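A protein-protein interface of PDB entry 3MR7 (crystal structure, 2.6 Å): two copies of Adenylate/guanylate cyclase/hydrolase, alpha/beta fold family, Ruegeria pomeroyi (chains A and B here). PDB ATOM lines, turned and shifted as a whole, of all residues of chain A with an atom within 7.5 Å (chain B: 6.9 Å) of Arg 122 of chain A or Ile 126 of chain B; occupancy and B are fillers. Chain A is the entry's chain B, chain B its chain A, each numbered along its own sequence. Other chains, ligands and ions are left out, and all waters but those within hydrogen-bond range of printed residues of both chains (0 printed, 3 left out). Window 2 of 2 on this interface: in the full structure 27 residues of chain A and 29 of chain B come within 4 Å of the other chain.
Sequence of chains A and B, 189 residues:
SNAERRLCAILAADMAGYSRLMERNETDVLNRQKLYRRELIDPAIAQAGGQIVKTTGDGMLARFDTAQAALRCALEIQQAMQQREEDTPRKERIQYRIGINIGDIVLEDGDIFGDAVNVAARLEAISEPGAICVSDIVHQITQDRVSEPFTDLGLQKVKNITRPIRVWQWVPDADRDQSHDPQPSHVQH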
ATOM      1  N   ALA A  12       1.409  25.767 -16.634  1.00  0.00           N
ATOM      2  CA  ALA A  12       0.375  26.001 -15.629  1.00  0.00           C
ATOM      3  C   ALA A  12       0.826  27.154 -14.765  1.00  0.00           C
ATOM      4  O   ALA A  12       1.996  27.282 -14.475  1.00  0.00           O
ATOM      5  CB  ALA A  12       0.137  24.753 -14.795  1.00  0.00           C
ATOM      6  N   ARG A  97       3.178  31.215  -9.357  1.00  0.00           N
ATOM      7  CA  ARG A  97       3.976  30.006  -9.464  1.00  0.00           C
ATOM      8  C   ARG A  97       3.702  29.516 -10.867  1.00  0.00           C
ATOM      9  O   ARG A  97       2.568  29.630 -11.348  1.00  0.00           O
ATOM     10  CB  ARG A  97       3.522  28.942  -8.475  1.00  0.00           C
ATOM     11  CG  ARG A  97       3.581  29.347  -7.045  1.00  0.00           C
ATOM     12  CD  ARG A  97       3.336  28.158  -6.138  1.00  0.00           C
ATOM     13  NE  ARG A  97       1.996  27.601  -6.284  1.00  0.00           N
ATOM     14  CZ  ARG A  97       0.929  28.092  -5.670  1.00  0.00           C
ATOM     15  NH1 ARG A  97       1.051  29.138  -4.869  1.00  0.00           N
ATOM     16  NH2 ARG A  97      -0.255  27.543  -5.850  1.00  0.00           N
ATOM     17  N   GLY A  99       4.550  26.134 -13.646  1.00  0.00           N
ATOM     18  CA  GLY A  99       5.090  24.832 -13.989  1.00  0.00           C
ATOM     19  C   GLY A  99       5.042  24.586 -15.489  1.00  0.00           C
ATOM     20  O   GLY A  99       4.147  25.041 -16.182  1.00  0.00           O
ATOM     21  N   ALA A 116       0.598  14.485 -18.902  1.00  0.00           N
ATOM     22  CA  ALA A 116       1.601  15.540 -18.961  1.00  0.00           C
ATOM     23  C   ALA A 116       0.982  16.856 -18.480  1.00  0.00           C
ATOM     24  O   ALA A 116       1.665  17.706 -17.905  1.00  0.00           O
ATOM     25  CB  ALA A 116       2.221  15.655 -20.380  1.00  0.00           C
ATOM     26  N   VAL A 117      -0.329  16.993 -18.668  1.00  0.00           N
ATOM     27  CA  VAL A 117      -1.063  18.146 -18.166  1.00  0.00           C
ATOM     28  C   VAL A 117      -1.123  18.180 -16.649  1.00  0.00           C
ATOM     29  O   VAL A 117      -0.921  19.219 -16.027  1.00  0.00           O
ATOM     30  CB  VAL A 117      -2.497  18.139 -18.649  1.00  0.00           C
ATOM     31  CG1 VAL A 117      -3.240  19.198 -17.932  1.00  0.00           C
ATOM     32  CG2 VAL A 117      -2.550  18.365 -20.146  1.00  0.00           C
ATOM     33  N   ASN A 118      -1.417  17.041 -16.045  1.00  0.00           N
ATOM     34  CA  ASN A 118      -1.543  16.990 -14.603  1.00  0.00           C
ATOM     35  C   ASN A 118      -0.208  17.225 -13.931  1.00  0.00           C
ATOM     36  O   ASN A 118      -0.139  17.902 -12.902  1.00  0.00           O
ATOM     37  CB  ASN A 118      -2.127  15.667 -14.174  1.00  0.00           C
ATOM     38  CG  ASN A 118      -3.551  15.501 -14.636  1.00  0.00           C
ATOM     39  OD1 ASN A 118      -4.082  16.354 -15.345  1.00  0.00           O
ATOM     40  ND2 ASN A 118      -4.182  14.414 -14.232  1.00  0.00           N
ATOM     41  N   VAL A 119       0.840  16.676 -14.539  1.00  0.00           N
ATOM     42  CA  VAL A 119       2.207  16.917 -14.123  1.00  0.00           C
ATOM     43  C   VAL A 119       2.566  18.407 -14.180  1.00  0.00           C
ATOM     44  O   VAL A 119       3.279  18.919 -13.301  1.00  0.00           O
ATOM     45  CB  VAL A 119       3.215  16.168 -15.012  1.00  0.00           C
ATOM     46  CG1 VAL A 119       4.577  16.761 -14.863  1.00  0.00           C
ATOM     47  CG2 VAL A 119       3.269  14.760 -14.663  1.00  0.00           C
ATOM     48  N   ALA A 120       2.110  19.105 -15.212  1.00  0.00           N
ATOM     49  CA  ALA A 120       2.446  20.518 -15.307  1.00  0.00           C
ATOM     50  C   ALA A 120       1.738  21.272 -14.174  1.00  0.00           C
ATOM     51  O   ALA A 120       2.290  22.209 -13.587  1.00  0.00           O
ATOM     52  CB  ALA A 120       2.061  21.053 -16.627  1.00  0.00           C
ATOM     53  N   ALA A 121       0.530  20.835 -13.835  1.00  0.00           N
ATOM     54  CA  ALA A 121      -0.240  21.449 -12.743  1.00  0.00           C
ATOM     55  C   ALA A 121       0.403  21.226 -11.371  1.00  0.00           C
ATOM     56  O   ALA A 121       0.376  22.121 -10.512  1.00  0.00           O
ATOM     57  CB  ALA A 121      -1.663  20.915 -12.738  1.00  0.00           C
ATOM     58  N   ARG A 122       0.959  20.025 -11.170  1.00  0.00           N
ATOM     59  CA  ARG A 122       1.716  19.692  -9.950  1.00  0.00           C
ATOM     60  C   ARG A 122       2.984  20.544  -9.800  1.00  0.00           C
ATOM     61  O   ARG A 122       3.290  21.028  -8.709  1.00  0.00           O
ATOM     62  CB  ARG A 122       2.041  18.196  -9.882  1.00  0.00           C
ATOM     63  CG  ARG A 122       2.729  17.729  -8.621  1.00  0.00           C
ATOM     64  CD  ARG A 122       1.937  18.127  -7.403  1.00  0.00           C
ATOM     65  NE  ARG A 122       2.649  17.849  -6.156  1.00  0.00           N
ATOM     66  CZ  ARG A 122       2.162  18.120  -4.949  1.00  0.00           C
ATOM     67  NH1 ARG A 122       0.963  18.680  -4.823  1.00  0.00           N
ATOM     68  NH2 ARG A 122       2.868  17.826  -3.870  1.00  0.00           N
ATOM     69  N   LEU A 123       3.688  20.779 -10.899  1.00  0.00           N
ATOM     70  CA  LEU A 123       4.897  21.590 -10.834  1.00  0.00           C
ATOM     71  C   LEU A 123       4.533  22.997 -10.453  1.00  0.00           C
ATOM     72  O   LEU A 123       5.248  23.658  -9.723  1.00  0.00           O
ATOM     73  CB  LEU A 123       5.649  21.585 -12.162  1.00  0.00           C
ATOM     74  CG  LEU A 123       6.171  20.191 -12.496  1.00  0.00           C
ATOM     75  CD1 LEU A 123       6.938  20.199 -13.786  1.00  0.00           C
ATOM     76  CD2 LEU A 123       7.040  19.722 -11.360  1.00  0.00           C
ATOM     77  N   GLU A 124       3.406  23.464 -10.954  1.00  0.00           N
ATOM     78  CA  GLU A 124       2.995  24.809 -10.635  1.00  0.00           C
ATOM     79  C   GLU A 124       2.706  24.872  -9.119  1.00  0.00           C
ATOM     80  O   GLU A 124       3.182  25.756  -8.401  1.00  0.00           O
ATOM     81  CB  GLU A 124       1.802  25.183 -11.532  1.00  0.00           C
ATOM     82  CG  GLU A 124       1.055  26.432 -11.178  1.00  0.00           C
ATOM     83  CD  GLU A 124       0.211  26.231  -9.938  1.00  0.00           C
ATOM     84  OE1 GLU A 124      -0.730  25.390  -9.969  1.00  0.00           O
ATOM     85  OE2 GLU A 124       0.504  26.918  -8.935  1.00  0.00           O
ATOM     86  N   ALA A 125       1.967  23.890  -8.640  1.00  0.00           N
ATOM     87  CA  ALA A 125       1.599  23.817  -7.243  1.00  0.00           C
ATOM     88  C   ALA A 125       2.786  23.892  -6.291  1.00  0.00           C
ATOM     89  O   ALA A 125       2.706  24.594  -5.286  1.00  0.00           O
ATOM     90  CB  ALA A 125       0.790  22.550  -6.975  1.00  0.00           C
ATOM     91  N   ILE A 126       3.877  23.182  -6.595  1.00  0.00           N
ATOM     92  CA  ILE A 126       4.991  23.010  -5.636  1.00  0.00           C
ATOM     93  C   ILE A 126       6.130  24.019  -5.872  1.00  0.00           C
ATOM     94  O   ILE A 126       7.153  24.020  -5.191  1.00  0.00           O
ATOM     95  CB  ILE A 126       5.613  21.608  -5.728  1.00  0.00           C
ATOM     96  CG1 ILE A 126       6.413  21.483  -7.029  1.00  0.00           C
ATOM     97  CG2 ILE A 126       4.552  20.511  -5.616  1.00  0.00           C
ATOM     98  CD1 ILE A 126       7.080  20.128  -7.215  1.00  0.00           C
ATOM     99  N   SER A 127       5.938  24.882  -6.848  1.00  0.00           N
ATOM    100  CA  SER A 127       6.967  25.796  -7.234  1.00  0.00           C
ATOM    101  C   SER A 127       7.018  26.922  -6.211  1.00  0.00           C
ATOM    102  O   SER A 127       6.045  27.221  -5.530  1.00  0.00           O
ATOM    103  CB  SER A 127       6.658  26.320  -8.641  1.00  0.00           C
ATOM    104  OG  SER A 127       7.490  27.405  -8.984  1.00  0.00           O
ATOM    105  N   CYS A 133       9.068  25.987 -12.097  1.00  0.00           N
ATOM    106  CA  CYS A 133       9.476  24.572 -12.041  1.00  0.00           C
ATOM    107  C   CYS A 133       9.174  23.858 -13.348  1.00  0.00           C
ATOM    108  O   CYS A 133       8.068  23.960 -13.865  1.00  0.00           O
ATOM    109  CB  CYS A 133       8.797  23.829 -10.897  1.00  0.00           C
ATOM    110  SG  CYS A 133       9.541  24.123  -9.277  1.00  0.00           S
ATOM    111  N   GLN A 156       9.794  13.643  -7.699  1.00  0.00           N
ATOM    112  CA  GLN A 156       8.570  14.146  -7.125  1.00  0.00           C
ATOM    113  C   GLN A 156       7.405  13.232  -7.463  1.00  0.00           C
ATOM    114  O   GLN A 156       7.040  13.090  -8.621  1.00  0.00           O
ATOM    115  CB  GLN A 156       8.312  15.534  -7.683  1.00  0.00           C
ATOM    116  CG  GLN A 156       7.558  16.426  -6.760  1.00  0.00           C
ATOM    117  CD  GLN A 156       8.449  17.018  -5.726  1.00  0.00           C
ATOM    118  OE1 GLN A 156       8.063  17.145  -4.583  1.00  0.00           O
ATOM    119  NE2 GLN A 156       9.659  17.375  -6.115  1.00  0.00           N
ATOM    120  N   LYS A 157       6.813  12.609  -6.453  1.00  0.00           N
ATOM    121  CA  LYS A 157       5.649  11.791  -6.721  1.00  0.00           C
ATOM    122  C   LYS A 157       4.517  12.699  -7.138  1.00  0.00           C
ATOM    123  O   LYS A 157       4.129  13.602  -6.394  1.00  0.00           O
ATOM    124  CB  LYS A 157       5.250  10.972  -5.500  1.00  0.00           C
ATOM    125  CG  LYS A 157       4.021  10.097  -5.727  1.00  0.00           C
ATOM    126  CD  LYS A 157       4.305   8.983  -6.741  1.00  0.00           C
ATOM    127  CE  LYS A 157       3.027   8.322  -7.195  1.00  0.00           C
ATOM    128  NZ  LYS A 157       1.933   8.702  -6.285  1.00  0.00           N
ATOM    129  N   VAL A 158       3.996  12.483  -8.338  1.00  0.00           N
ATOM    130  CA  VAL A 158       2.769  13.161  -8.733  1.00  0.00           C
ATOM    131  C   VAL A 158       1.584  12.223  -8.525  1.00  0.00           C
ATOM    132  O   VAL A 158       1.661  11.028  -8.850  1.00  0.00           O
ATOM    133  CB  VAL A 158       2.808  13.593 -10.196  1.00  0.00           C
ATOM    134  CG1 VAL A 158       1.447  14.198 -10.615  1.00  0.00           C
ATOM    135  CG2 VAL A 158       3.934  14.549 -10.400  1.00  0.00           C
ATOM    136  N   LYS A 159       0.491  12.761  -7.987  1.00  0.00           N
ATOM    137  CA  LYS A 159      -0.684  11.951  -7.682  1.00  0.00           C
ATOM    138  C   LYS A 159      -1.200  11.130  -8.885  1.00  0.00           C
ATOM    139  O   LYS A 159      -1.323  11.639  -9.999  1.00  0.00           O
ATOM    140  CB  LYS A 159      -1.801  12.822  -7.131  1.00  0.00           C
ATOM    141  CG  LYS A 159      -3.120  12.072  -6.952  1.00  0.00           C
ATOM    142  CD  LYS A 159      -4.165  13.033  -6.484  1.00  0.00           C
ATOM    143  CE  LYS A 159      -5.419  12.350  -6.038  1.00  0.00           C
ATOM    144  NZ  LYS A 159      -6.345  13.424  -5.581  1.00  0.00           N
ATOM    145  N   VAL A 167      12.329  17.196 -11.016  1.00  0.00           N
ATOM    146  CA  VAL A 167      11.918  18.578 -11.195  1.00  0.00           C
ATOM    147  C   VAL A 167      13.068  19.547 -11.071  1.00  0.00           C
ATOM    148  O   VAL A 167      13.885  19.451 -10.157  1.00  0.00           O
ATOM    149  CB  VAL A 167      10.908  18.955 -10.148  1.00  0.00           C
ATOM    150  CG1 VAL A 167      10.501  20.436 -10.285  1.00  0.00           C
ATOM    151  CG2 VAL A 167       9.734  18.051 -10.273  1.00  0.00           C
ATOM    152  N   ARG B  97      -5.177  21.999   3.177  1.00  0.00           N
ATOM    153  CA  ARG B  97      -3.925  21.215   3.135  1.00  0.00           C
ATOM    154  C   ARG B  97      -3.310  21.326   4.521  1.00  0.00           C
ATOM    155  O   ARG B  97      -3.448  22.361   5.167  1.00  0.00           O
ATOM    156  CB  ARG B  97      -2.944  21.774   2.089  1.00  0.00           C
ATOM    157  CG  ARG B  97      -3.312  21.484   0.639  1.00  0.00           C
ATOM    158  CD  ARG B  97      -2.163  21.825  -0.230  1.00  0.00           C
ATOM    159  NE  ARG B  97      -1.765  23.181   0.075  1.00  0.00           N
ATOM    160  CZ  ARG B  97      -2.150  24.228  -0.634  1.00  0.00           C
ATOM    161  NH1 ARG B  97      -2.899  24.039  -1.706  1.00  0.00           N
ATOM    162  NH2 ARG B  97      -1.792  25.456  -0.275  1.00  0.00           N
ATOM    163  N   ALA B 121       5.511  24.384   7.267  1.00  0.00           N
ATOM    164  CA  ALA B 121       4.889  25.223   6.251  1.00  0.00           C
ATOM    165  C   ALA B 121       5.007  24.604   4.873  1.00  0.00           C
ATOM    166  O   ALA B 121       4.044  24.583   4.106  1.00  0.00           O
ATOM    167  CB  ALA B 121       5.562  26.572   6.254  1.00  0.00           C
ATOM    168  N   ARG B 122       6.206  24.122   4.556  1.00  0.00           N
ATOM    169  CA  ARG B 122       6.466  23.464   3.284  1.00  0.00           C
ATOM    170  C   ARG B 122       5.636  22.183   3.144  1.00  0.00           C
ATOM    171  O   ARG B 122       5.081  21.900   2.082  1.00  0.00           O
ATOM    172  CB  ARG B 122       7.955  23.171   3.151  1.00  0.00           C
ATOM    173  CG  ARG B 122       8.357  22.705   1.785  1.00  0.00           C
ATOM    174  CD  ARG B 122       7.841  23.657   0.736  1.00  0.00           C
ATOM    175  NE  ARG B 122       8.038  23.018  -0.542  1.00  0.00           N
ATOM    176  CZ  ARG B 122       7.596  23.455  -1.703  1.00  0.00           C
ATOM    177  NH1 ARG B 122       6.873  24.568  -1.779  1.00  0.00           N
ATOM    178  NH2 ARG B 122       7.874  22.741  -2.790  1.00  0.00           N
ATOM    179  N   LEU B 123       5.530  21.420   4.226  1.00  0.00           N
ATOM    180  CA  LEU B 123       4.721  20.214   4.211  1.00  0.00           C
ATOM    181  C   LEU B 123       3.283  20.534   3.856  1.00  0.00           C
ATOM    182  O   LEU B 123       2.657  19.820   3.080  1.00  0.00           O
ATOM    183  CB  LEU B 123       4.830  19.483   5.545  1.00  0.00           C
ATOM    184  CG  LEU B 123       5.856  18.327   5.585  1.00  0.00           C
ATOM    185  CD1 LEU B 123       6.994  18.555   4.604  1.00  0.00           C
ATOM    186  CD2 LEU B 123       6.399  18.079   6.988  1.00  0.00           C
ATOM    187  N   GLU B 124       2.765  21.623   4.413  1.00  0.00           N
ATOM    188  CA  GLU B 124       1.424  22.080   4.093  1.00  0.00           C
ATOM    189  C   GLU B 124       1.341  22.331   2.582  1.00  0.00           C
ATOM    190  O   GLU B 124       0.463  21.857   1.897  1.00  0.00           O
ATOM    191  CB  GLU B 124       1.100  23.335   4.916  1.00  0.00           C
ATOM    192  CG  GLU B 124      -0.149  24.119   4.470  1.00  0.00           C
ATOM    193  CD  GLU B 124       0.088  24.983   3.221  1.00  0.00           C
ATOM    194  OE1 GLU B 124       0.879  25.969   3.265  1.00  0.00           O
ATOM    195  OE2 GLU B 124      -0.533  24.673   2.182  1.00  0.00           O
ATOM    196  N   ALA B 125       2.302  23.046   2.053  1.00  0.00           N
ATOM    197  CA  ALA B 125       2.234  23.476   0.671  1.00  0.00           C
ATOM    198  C   ALA B 125       2.287  22.322  -0.328  1.00  0.00           C
ATOM    199  O   ALA B 125       1.655  22.379  -1.367  1.00  0.00           O
ATOM    200  CB  ALA B 125       3.346  24.475   0.393  1.00  0.00           C
ATOM    201  N   ILE B 126       3.046  21.278  -0.038  1.00  0.00           N
ATOM    202  CA  ILE B 126       3.109  20.167  -0.977  1.00  0.00           C
ATOM    203  C   ILE B 126       2.058  19.108  -0.674  1.00  0.00           C
ATOM    204  O   ILE B 126       1.822  18.244  -1.496  1.00  0.00           O
ATOM    205  CB  ILE B 126       4.457  19.483  -0.940  1.00  0.00           C
ATOM    206  CG1 ILE B 126       4.542  18.695   0.378  1.00  0.00           C
ATOM    207  CG2 ILE B 126       5.603  20.519  -1.214  1.00  0.00           C
ATOM    208  CD1 ILE B 126       5.861  18.160   0.702  1.00  0.00           C
ATOM    209  N   SER B 127       1.424  19.174   0.492  1.00  0.00           N
ATOM    210  CA  SER B 127       0.394  18.205   0.851  1.00  0.00           C
ATOM    211  C   SER B 127      -0.722  18.187  -0.172  1.00  0.00           C
ATOM    212  O   SER B 127      -1.069  19.216  -0.720  1.00  0.00           O
ATOM    213  CB  SER B 127      -0.214  18.558   2.202  1.00  0.00           C
ATOM    214  OG  SER B 127      -1.343  17.749   2.453  1.00  0.00           O
ATOM    215  N   GLU B 128      -1.324  17.041  -0.435  1.00  0.00           N
ATOM    216  CA  GLU B 128      -2.437  17.140  -1.337  1.00  0.00           C
ATOM    217  C   GLU B 128      -3.695  17.617  -0.650  1.00  0.00           C
ATOM    218  O   GLU B 128      -3.829  17.524   0.557  1.00  0.00           O
ATOM    219  CB  GLU B 128      -2.605  15.952  -2.279  1.00  0.00           C
ATOM    220  CG  GLU B 128      -3.114  14.665  -1.757  1.00  0.00           C
ATOM    221  CD  GLU B 128      -2.930  13.574  -2.820  1.00  0.00           C
ATOM    222  OE1 GLU B 128      -2.035  13.743  -3.687  1.00  0.00           O
ATOM    223  OE2 GLU B 128      -3.671  12.566  -2.805  1.00  0.00           O
ATOM    224  N   PRO B 129      -4.588  18.217  -1.423  1.00  0.00           N
ATOM    225  CA  PRO B 129      -5.746  18.857  -0.815  1.00  0.00           C
ATOM    226  C   PRO B 129      -6.562  17.832  -0.076  1.00  0.00           C
ATOM    227  O   PRO B 129      -6.788  16.740  -0.597  1.00  0.00           O
ATOM    228  CB  PRO B 129      -6.513  19.386  -2.013  1.00  0.00           C
ATOM    229  CG  PRO B 129      -5.446  19.594  -3.073  1.00  0.00           C
ATOM    230  CD  PRO B 129      -4.533  18.430  -2.881  1.00  0.00           C
ATOM    231  N   CYS B 133       0.298  16.015   5.462  1.00  0.00           N
ATOM    232  CA  CYS B 133       1.685  15.574   5.283  1.00  0.00           C
ATOM    233  C   CYS B 133       2.470  15.802   6.559  1.00  0.00           C
ATOM    234  O   CYS B 133       2.404  16.876   7.137  1.00  0.00           O
ATOM    235  CB  CYS B 133       2.354  16.313   4.131  1.00  0.00           C
ATOM    236  SG  CYS B 133       1.950  15.650   2.530  1.00  0.00           S
ATOM    237  N   LEU B 153       6.431   9.306   0.924  1.00  0.00           N
ATOM    238  CA  LEU B 153       6.340  10.133  -0.265  1.00  0.00           C
ATOM    239  C   LEU B 153       7.722  10.429  -0.817  1.00  0.00           C
ATOM    240  O   LEU B 153       7.850  11.032  -1.861  1.00  0.00           O
ATOM    241  CB  LEU B 153       5.701  11.459   0.110  1.00  0.00           C
ATOM    242  CG  LEU B 153       4.525  11.807  -0.759  1.00  0.00           C
ATOM    243  CD1 LEU B 153       3.640  10.587  -0.824  1.00  0.00           C
ATOM    244  CD2 LEU B 153       3.807  12.999  -0.181  1.00  0.00           C
ATOM    245  N   GLN B 156      12.118  15.610   0.142  1.00  0.00           N
ATOM    246  CA  GLN B 156      11.601  16.908  -0.190  1.00  0.00           C
ATOM    247  C   GLN B 156      12.668  17.919   0.193  1.00  0.00           C
ATOM    248  O   GLN B 156      13.071  17.989   1.360  1.00  0.00           O
ATOM    249  CB  GLN B 156      10.359  17.129   0.639  1.00  0.00           C
ATOM    250  CG  GLN B 156       9.261  17.746  -0.083  1.00  0.00           C
ATOM    251  CD  GLN B 156       8.905  16.969  -1.285  1.00  0.00           C
ATOM    252  OE1 GLN B 156       8.987  15.736  -1.297  1.00  0.00           O
ATOM    253  NE2 GLN B 156       8.514  17.677  -2.328  1.00  0.00           N
ATOM    254  N   LYS B 157      13.160  18.676  -0.778  1.00  0.00           N
ATOM    255  CA  LYS B 157      14.122  19.715  -0.450  1.00  0.00           C
ATOM    256  C   LYS B 157      13.331  20.942  -0.041  1.00  0.00           C
ATOM    257  O   LYS B 157      12.305  21.223  -0.606  1.00  0.00           O
ATOM    258  CB  LYS B 157      15.070  19.978  -1.627  1.00  0.00           C
ATOM    259  CG  LYS B 157      15.608  21.380  -1.716  1.00  0.00           C
ATOM    260  CD  LYS B 157      16.749  21.690  -0.743  1.00  0.00           C
ATOM    261  CE  LYS B 157      16.946  23.218  -0.721  1.00  0.00           C
ATOM    262  NZ  LYS B 157      18.138  23.730   0.028  1.00  0.00           N
ATOM    263  N   VAL B 167       8.957  12.667   3.696  1.00  0.00           N
ATOM    264  CA  VAL B 167       7.603  13.105   3.947  1.00  0.00           C
ATOM    265  C   VAL B 167       6.597  11.963   3.808  1.00  0.00           C
ATOM    266  O   VAL B 167       6.595  11.216   2.822  1.00  0.00           O
ATOM    267  CB  VAL B 167       7.263  14.270   2.978  1.00  0.00           C
ATOM    268  CG1 VAL B 167       5.799  14.626   3.012  1.00  0.00           C
ATOM    269  CG2 VAL B 167       8.140  15.486   3.310  1.00  0.00           C
ATOM    270  N   GLN B 169       2.478  10.848   3.971  1.00  0.00           N
ATOM    271  CA  GLN B 169       1.184  11.438   3.686  1.00  0.00           C
ATOM    272  C   GLN B 169       0.014  10.515   3.937  1.00  0.00           C
ATOM    273  O   GLN B 169       0.054   9.319   3.671  1.00  0.00           O
ATOM    274  CB  GLN B 169       1.121  11.915   2.234  1.00  0.00           C
ATOM    275  CG  GLN B 169      -0.161  12.653   1.885  1.00  0.00           C
ATOM    276  CD  GLN B 169      -0.165  13.122   0.460  1.00  0.00           C
ATOM    277  OE1 GLN B 169      -0.246  12.310  -0.461  1.00  0.00           O
ATOM    278  NE2 GLN B 169      -0.064  14.435   0.258  1.00  0.00           N
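The backbone carbonyl oxygen of Ile 126 of chain A is in hydrogen-bond range of the guanidinium group of Arg 122 of chain B, at 2.8 Å.
The backbone carbonyl oxygen of Ile 126 of chain B sits at hydrogen-bond distance from the guanidinium group of Arg 122 of chain A.
The side-chain amino group of Lys 159 of chain A is in salt-bridge range of the side-chain carboxylate of Glu 128 of chain B, at 3.9 Å.
The side-chain amide oxygen (OE1) of Gln 156 of chain A lies close to the side-chain amide nitrogen (NE2) of Gln 156 of chain B.
The side-chain amide nitrogen (NE2) of Gln 169 of chain B sits close to the backbone NH (N) of Glu 128 of chain B, 3.0 Å away.
No residue of chain A comes within 4 Å of Ala 125 of chain B.
Printed residues of chain B within 4 Å of Lys 159 of chain A: Glu 128 (3.6 Å).
Printed residues of chain A within 4 Å of Arg 122 of chain B: Ile 126 (2.8 Å).
Pro 129 of chain B touches none of the printed residues of chain A.
The nearest residue of chain B that does not touch Arg 122 of chain A is Ser 127 of chain B (4.6 Å).
The nearest residue of chain A that does not touch Ile 126 of chain B is Ile 126 of chain A (4.5 Å).
The nearest printed residue of chain B that does not touch Lys 159 of chain A is Pro 129 of chain B (6.0 Å).
Printed residues of chain B that touch a printed residue of chain A: Arg 122, Ile 126, Glu 128 and Gln 156.
Hydrophobic or aromatic side chains of chain A within 4 Å of the printed part of chain B: Ile 126.
Among the printed residues, 4 pairs touch across the chains.
Among the printed residues, Asp or Glu carboxylates within 4 Å of a Lys or Arg side-chain nitrogen of the other chain: Lys 159 of chain A with Glu 128 of chain B (3.9 Å).
Arg 122 of chain A touches Ile 126 of chain B, and with the chains exchanged Ile 126 of chain A touches Arg 122 of chain B.
Gln 156 of chain B touches its own counterpart, Gln 156 of chain A.
Positions printed for both chains: 97, 121, 122, 123, 124, 125, 126, 127, 133, 156, 157 and 167.
Of the 4 pairs that touch across the chains among the printed residues, 3 have their exchanged pair printed and touching as well.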
